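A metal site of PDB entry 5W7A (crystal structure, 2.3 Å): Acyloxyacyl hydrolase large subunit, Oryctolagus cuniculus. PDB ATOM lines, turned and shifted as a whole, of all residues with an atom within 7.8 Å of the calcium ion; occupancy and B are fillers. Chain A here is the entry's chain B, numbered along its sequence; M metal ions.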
ATOM      1  N   CYS A  52     -18.008  31.374  28.131  1.00  0.00           N
ATOM      2  CA  CYS A  52     -19.301  31.033  27.538  1.00  0.00           C
ATOM      3  C   CYS A  52     -20.376  30.757  28.588  1.00  0.00           C
ATOM      4  O   CYS A  52     -21.549  30.624  28.216  1.00  0.00           O
ATOM      5  CB  CYS A  52     -19.154  29.822  26.601  1.00  0.00           C
ATOM      6  SG  CYS A  52     -18.471  28.299  27.328  1.00  0.00           S
ATOM      7  N   ARG A  63     -10.582  23.868  29.596  1.00  0.00           N
ATOM      8  CA  ARG A  63     -10.941  22.757  30.457  1.00  0.00           C
ATOM      9  C   ARG A  63     -11.070  21.470  29.649  1.00  0.00           C
ATOM     10  O   ARG A  63     -11.463  21.492  28.475  1.00  0.00           O
ATOM     11  CB  ARG A  63     -12.251  23.048  31.182  1.00  0.00           C
ATOM     12  CG  ARG A  63     -12.630  22.067  32.265  1.00  0.00           C
ATOM     13  CD  ARG A  63     -13.974  22.453  32.842  1.00  0.00           C
ATOM     14  NE  ARG A  63     -14.524  21.471  33.773  1.00  0.00           N
ATOM     15  CZ  ARG A  63     -14.275  21.450  35.082  1.00  0.00           C
ATOM     16  NH1 ARG A  63     -13.479  22.356  35.638  1.00  0.00           N
ATOM     17  NH2 ARG A  63     -14.837  20.518  35.845  1.00  0.00           N
ATOM     18  N   ARG A  64     -10.717  20.353  30.257  1.00  0.00           N
ATOM     19  CA  ARG A  64     -11.025  19.081  29.646  1.00  0.00           C
ATOM     20  C   ARG A  64     -12.539  18.898  29.609  1.00  0.00           C
ATOM     21  O   ARG A  64     -13.229  19.289  30.556  1.00  0.00           O
ATOM     22  CB  ARG A  64     -10.372  17.909  30.396  1.00  0.00           C
ATOM     23  CG  ARG A  64      -8.842  17.904  30.354  1.00  0.00           C
ATOM     24  CD  ARG A  64      -8.274  16.485  30.455  1.00  0.00           C
ATOM     25  NE  ARG A  64      -7.292  16.346  31.520  1.00  0.00           N
ATOM     26  CZ  ARG A  64      -5.993  16.672  31.428  1.00  0.00           C
ATOM     27  NH1 ARG A  64      -5.491  17.173  30.307  1.00  0.00           N
ATOM     28  NH2 ARG A  64      -5.205  16.483  32.475  1.00  0.00           N
ATOM     29  N   PRO A  65     -13.094  18.339  28.540  1.00  0.00           N
ATOM     30  CA  PRO A  65     -14.545  18.201  28.465  1.00  0.00           C
ATOM     31  C   PRO A  65     -15.070  17.205  29.487  1.00  0.00           C
ATOM     32  O   PRO A  65     -14.478  16.137  29.695  1.00  0.00           O
ATOM     33  CB  PRO A  65     -14.797  17.692  27.039  1.00  0.00           C
ATOM     34  CG  PRO A  65     -13.541  17.969  26.303  1.00  0.00           C
ATOM     35  CD  PRO A  65     -12.445  17.876  27.297  1.00  0.00           C
ATOM     36  N   ASP A  66     -16.171  17.566  30.128  1.00  0.00           N
ATOM     37  CA  ASP A  66     -16.847  16.680  31.070  1.00  0.00           C
ATOM     38  C   ASP A  66     -17.829  15.826  30.283  1.00  0.00           C
ATOM     39  O   ASP A  66     -18.822  16.334  29.762  1.00  0.00           O
ATOM     40  CB  ASP A  66     -17.560  17.494  32.152  1.00  0.00           C
ATOM     41  CG  ASP A  66     -18.328  16.613  33.121  1.00  0.00           C
ATOM     42  OD1 ASP A  66     -19.555  16.452  32.916  1.00  0.00           O
ATOM     43  OD2 ASP A  66     -17.706  16.086  34.073  1.00  0.00           O
ATOM     44  N   TRP A  68     -17.216  14.599  27.463  1.00  0.00           N
ATOM     45  CA  TRP A  68     -17.007  14.955  26.063  1.00  0.00           C
ATOM     46  C   TRP A  68     -18.009  15.999  25.571  1.00  0.00           C
ATOM     47  O   TRP A  68     -18.325  16.072  24.386  1.00  0.00           O
ATOM     48  CB  TRP A  68     -17.041  13.705  25.171  1.00  0.00           C
ATOM     49  CG  TRP A  68     -15.859  12.807  25.375  1.00  0.00           C
ATOM     50  CD1 TRP A  68     -15.825  11.637  26.072  1.00  0.00           C
ATOM     51  CD2 TRP A  68     -14.526  13.017  24.883  1.00  0.00           C
ATOM     52  NE1 TRP A  68     -14.549  11.099  26.045  1.00  0.00           N
ATOM     53  CE2 TRP A  68     -13.743  11.938  25.325  1.00  0.00           C
ATOM     54  CE3 TRP A  68     -13.920  14.025  24.122  1.00  0.00           C
ATOM     55  CZ2 TRP A  68     -12.382  11.819  25.020  1.00  0.00           C
ATOM     56  CZ3 TRP A  68     -12.572  13.906  23.815  1.00  0.00           C
ATOM     57  CH2 TRP A  68     -11.818  12.812  24.262  1.00  0.00           C
ATOM     58  N   ASP A  69     -18.515  16.825  26.491  1.00  0.00           N
ATOM     59  CA  ASP A  69     -19.455  17.900  26.143  1.00  0.00           C
ATOM     60  C   ASP A  69     -20.592  17.369  25.290  1.00  0.00           C
ATOM     61  O   ASP A  69     -21.002  17.978  24.301  1.00  0.00           O
ATOM     62  CB  ASP A  69     -18.725  19.045  25.434  1.00  0.00           C
ATOM     63  CG  ASP A  69     -17.859  19.856  26.381  1.00  0.00           C
ATOM     64  OD1 ASP A  69     -17.503  19.325  27.464  1.00  0.00           O
ATOM     65  OD2 ASP A  69     -17.513  21.009  26.056  1.00  0.00           O
ATOM     66  N   ALA A  70     -21.125  16.203  25.679  1.00  0.00           N
ATOM     67  CA  ALA A  70     -22.278  15.651  24.981  1.00  0.00           C
ATOM     68  C   ALA A  70     -23.528  16.489  25.229  1.00  0.00           C
ATOM     69  O   ALA A  70     -24.373  16.600  24.346  1.00  0.00           O
ATOM     70  CB  ALA A  70     -22.504  14.203  25.422  1.00  0.00           C
ATOM     71  N   ARG A  72     -23.351  19.819  27.066  1.00  0.00           N
ATOM     72  CA  ARG A  72     -23.085  21.253  27.056  1.00  0.00           C
ATOM     73  C   ARG A  72     -21.612  21.495  26.752  1.00  0.00           C
ATOM     74  O   ARG A  72     -20.777  20.588  26.850  1.00  0.00           O
ATOM     75  CB  ARG A  72     -23.470  21.902  28.396  1.00  0.00           C
ATOM     76  CG  ARG A  72     -22.579  21.565  29.586  1.00  0.00           C
ATOM     77  CD  ARG A  72     -22.926  22.474  30.759  1.00  0.00           C
ATOM     78  NE  ARG A  72     -22.023  22.311  31.900  1.00  0.00           N
ATOM     79  CZ  ARG A  72     -22.034  23.116  32.955  1.00  0.00           C
ATOM     80  NH1 ARG A  72     -22.874  24.148  33.007  1.00  0.00           N
ATOM     81  NH2 ARG A  72     -21.195  22.919  33.966  1.00  0.00           N
ATOM     82  N   ASP A  73     -21.320  22.734  26.376  1.00  0.00           N
ATOM     83  CA  ASP A  73     -19.962  23.157  26.073  1.00  0.00           C
ATOM     84  C   ASP A  73     -19.333  23.675  27.353  1.00  0.00           C
ATOM     85  O   ASP A  73     -19.644  24.785  27.796  1.00  0.00           O
ATOM     86  CB  ASP A  73     -19.968  24.212  24.968  1.00  0.00           C
ATOM     87  CG  ASP A  73     -18.594  24.471  24.405  1.00  0.00           C
ATOM     88  OD1 ASP A  73     -18.381  25.563  23.836  1.00  0.00           O
ATOM     89  OD2 ASP A  73     -17.735  23.572  24.525  1.00  0.00           O
ATOM     90  N   SER A  74     -18.451  22.874  27.953  1.00  0.00           N
ATOM     91  CA  SER A  74     -17.855  23.201  29.247  1.00  0.00           C
ATOM     92  C   SER A  74     -16.465  23.827  29.139  1.00  0.00           C
ATOM     93  O   SER A  74     -15.989  24.392  30.128  1.00  0.00           O
ATOM     94  CB  SER A  74     -17.763  21.944  30.113  1.00  0.00           C
ATOM     95  OG  SER A  74     -16.793  21.044  29.599  1.00  0.00           O
ATOM     96  N   ASN A  75     -15.811  23.727  27.980  1.00  0.00           N
ATOM     97  CA  ASN A  75     -14.503  24.341  27.781  1.00  0.00           C
ATOM     98  C   ASN A  75     -14.545  25.468  26.757  1.00  0.00           C
ATOM     99  O   ASN A  75     -13.486  25.952  26.335  1.00  0.00           O
ATOM    100  CB  ASN A  75     -13.467  23.282  27.386  1.00  0.00           C
ATOM    101  CG  ASN A  75     -13.819  22.560  26.102  1.00  0.00           C
ATOM    102  OD1 ASN A  75     -14.695  22.990  25.360  1.00  0.00           O
ATOM    103  ND2 ASN A  75     -13.116  21.474  25.821  1.00  0.00           N
ATOM    104  N   CYS A  76     -15.737  25.876  26.324  1.00  0.00           N
ATOM    105  CA  CYS A  76     -15.963  27.099  25.557  1.00  0.00           C
ATOM    106  C   CYS A  76     -15.279  27.104  24.184  1.00  0.00           C
ATOM    107  O   CYS A  76     -15.087  28.167  23.590  1.00  0.00           O
ATOM    108  CB  CYS A  76     -15.526  28.339  26.356  1.00  0.00           C
ATOM    109  SG  CYS A  76     -16.529  28.730  27.831  1.00  0.00           S
ATOM    110  N   ASN A  77     -14.940  25.935  23.632  1.00  0.00           N
ATOM    111  CA  ASN A  77     -14.372  25.881  22.282  1.00  0.00           C
ATOM    112  C   ASN A  77     -15.436  25.720  21.190  1.00  0.00           C
ATOM    113  O   ASN A  77     -15.082  25.496  20.028  1.00  0.00           O
ATOM    114  CB  ASN A  77     -13.328  24.769  22.180  1.00  0.00           C
ATOM    115  CG  ASN A  77     -13.918  23.370  22.303  1.00  0.00           C
ATOM    116  OD1 ASN A  77     -15.141  23.192  22.360  1.00  0.00           O
ATOM    117  ND2 ASN A  77     -13.041  22.367  22.338  1.00  0.00           N
ATOM    118  N   GLY A  78     -16.719  25.839  21.539  1.00  0.00           N
ATOM    119  CA  GLY A  78     -17.790  25.829  20.565  1.00  0.00           C
ATOM    120  C   GLY A  78     -18.208  24.446  20.101  1.00  0.00           C
ATOM    121  O   GLY A  78     -19.169  24.338  19.334  1.00  0.00           O
ATOM    122  N   ILE A  79     -17.524  23.405  20.554  1.00  0.00           N
ATOM    123  CA  ILE A  79     -17.809  22.036  20.147  1.00  0.00           C
ATOM    124  C   ILE A  79     -18.543  21.351  21.296  1.00  0.00           C
ATOM    125  O   ILE A  79     -18.082  21.384  22.443  1.00  0.00           O
ATOM    126  CB  ILE A  79     -16.508  21.297  19.790  1.00  0.00           C
ATOM    127  CG1 ILE A  79     -15.784  22.038  18.666  1.00  0.00           C
ATOM    128  CG2 ILE A  79     -16.801  19.869  19.370  1.00  0.00           C
ATOM    129  CD1 ILE A  79     -14.353  21.582  18.458  1.00  0.00           C
ATOM    130  N   TRP A  80     -19.695  20.747  20.991  1.00  0.00           N
ATOM    131  CA  TRP A  80     -20.510  20.088  22.005  1.00  0.00           C
ATOM    132  C   TRP A  80     -21.633  19.359  21.290  1.00  0.00           C
ATOM    133  O   TRP A  80     -21.816  19.472  20.080  1.00  0.00           O
ATOM    134  CB  TRP A  80     -21.064  21.062  23.034  1.00  0.00           C
ATOM    135  CG  TRP A  80     -22.056  22.047  22.481  1.00  0.00           C
ATOM    136  CD1 TRP A  80     -21.795  23.059  21.602  1.00  0.00           C
ATOM    137  CD2 TRP A  80     -23.469  22.106  22.741  1.00  0.00           C
ATOM    138  NE1 TRP A  80     -22.950  23.752  21.309  1.00  0.00           N
ATOM    139  CE2 TRP A  80     -23.986  23.180  21.997  1.00  0.00           C
ATOM    140  CE3 TRP A  80     -24.342  21.358  23.541  1.00  0.00           C
ATOM    141  CZ2 TRP A  80     -25.341  23.525  22.019  1.00  0.00           C
ATOM    142  CZ3 TRP A  80     -25.688  21.696  23.556  1.00  0.00           C
ATOM    143  CH2 TRP A  80     -26.169  22.773  22.813  1.00  0.00           C
ATOM    144  N   GLY A  81     -22.415  18.625  22.067  1.00  0.00           N
ATOM    145  CA  GLY A  81     -23.547  17.913  21.530  1.00  0.00           C
ATOM    146  C   GLY A  81     -23.146  16.548  21.022  1.00  0.00           C
ATOM    147  O   GLY A  81     -22.080  16.004  21.343  1.00  0.00           O
ATOM    148  N   GLU A  91     -17.358  16.529  20.155  1.00  0.00           N
ATOM    149  CA  GLU A  91     -15.987  16.832  20.557  1.00  0.00           C
ATOM    150  C   GLU A  91     -15.111  15.579  20.613  1.00  0.00           C
ATOM    151  O   GLU A  91     -13.886  15.690  20.535  1.00  0.00           O
ATOM    152  CB  GLU A  91     -15.948  17.555  21.920  1.00  0.00           C
ATOM    153  CG  GLU A  91     -14.531  18.079  22.267  1.00  0.00           C
ATOM    154  CD  GLU A  91     -14.492  19.276  23.222  1.00  0.00           C
ATOM    155  OE1 GLU A  91     -13.390  19.558  23.744  1.00  0.00           O
ATOM    156  OE2 GLU A  91     -15.526  19.929  23.437  1.00  0.00           O
ATOM    157  N   CYS A  95     -12.063  15.992  18.363  1.00  0.00           N
ATOM    158  CA  CYS A  95     -10.992  16.460  19.242  1.00  0.00           C
ATOM    159  C   CYS A  95     -10.395  15.380  20.125  1.00  0.00           C
ATOM    160  O   CYS A  95      -9.532  15.692  20.945  1.00  0.00           O
ATOM    161  CB  CYS A  95     -11.488  17.608  20.142  1.00  0.00           C
ATOM    162  SG  CYS A  95     -12.153  19.029  19.257  1.00  0.00           S
ATOM    163  N   CYS A 175      -9.987  22.913  18.000  1.00  0.00           N
ATOM    164  CA  CYS A 175     -10.440  22.603  19.340  1.00  0.00           C
ATOM    165  C   CYS A 175      -9.906  23.610  20.352  1.00  0.00           C
ATOM    166  O   CYS A 175     -10.533  23.814  21.405  1.00  0.00           O
ATOM    167  CB  CYS A 175     -10.009  21.179  19.716  1.00  0.00           C
ATOM    168  SG  CYS A 175     -10.503  19.939  18.495  1.00  0.00           S
HETATM  169 CA    CA M   1     -16.503  21.881  24.073  1.00  0.00          CA
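Of the 21 residues printed, 6 come within 4 Å of the calcium ion.
Along chain A the residues within 4 Å of the calcium ion span positions 69 to 91.
The backbone NH (N) of Gly 78 is in hydrogen-bond range of the side-chain carboxylate (OD1) of Asp 73.
The side-chain carboxylate (OD1) of Asp 69 is in hydrogen-bond range of the backbone NH (N) of Asp 66, at 3.5 Å.
The side-chain amide nitrogen (ND2) of Asn 75 sits close to the backbone carbonyl oxygen (O) of Arg 63 (3.1 Å).
The backbone carbonyl oxygen of Cys 175 lies within hydrogen-bond range of the side-chain amide nitrogen of Asn 77 (3.0 Å).
The side-chain sulfur of Cys 175 is disulfide-bonded to the side-chain sulfur of Cys 95 (2.0 Å).
SG of Cys 76 is disulfide-bonded to SG of Cys 52 (2.1 Å).
OD1 of Asp 69 sits at hydrogen-bond distance from OG of Ser 74 (2.8 Å).
The backbone carbonyl oxygen (O) of Asp 69 is in hydrogen-bond range of the backbone NH (N) of Gly 81, 2.7 Å away.
OD2 of Asp 73 binds the calcium ion (2.1 Å).
The calcium ion is bound by OE2 of Glu 91, at 2.3 Å.
The calcium ion is bound by the backbone carbonyl oxygen (O) of Ile 79 (2.3 Å).
OD2 of Asp 69 binds the calcium ion (2.4 Å).
The calcium ion is bound by OD1 of Asn 75 (2.5 Å).
The side-chain amide oxygen (OD1) of Asn 77 is bound to the calcium ion (2.6 Å).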
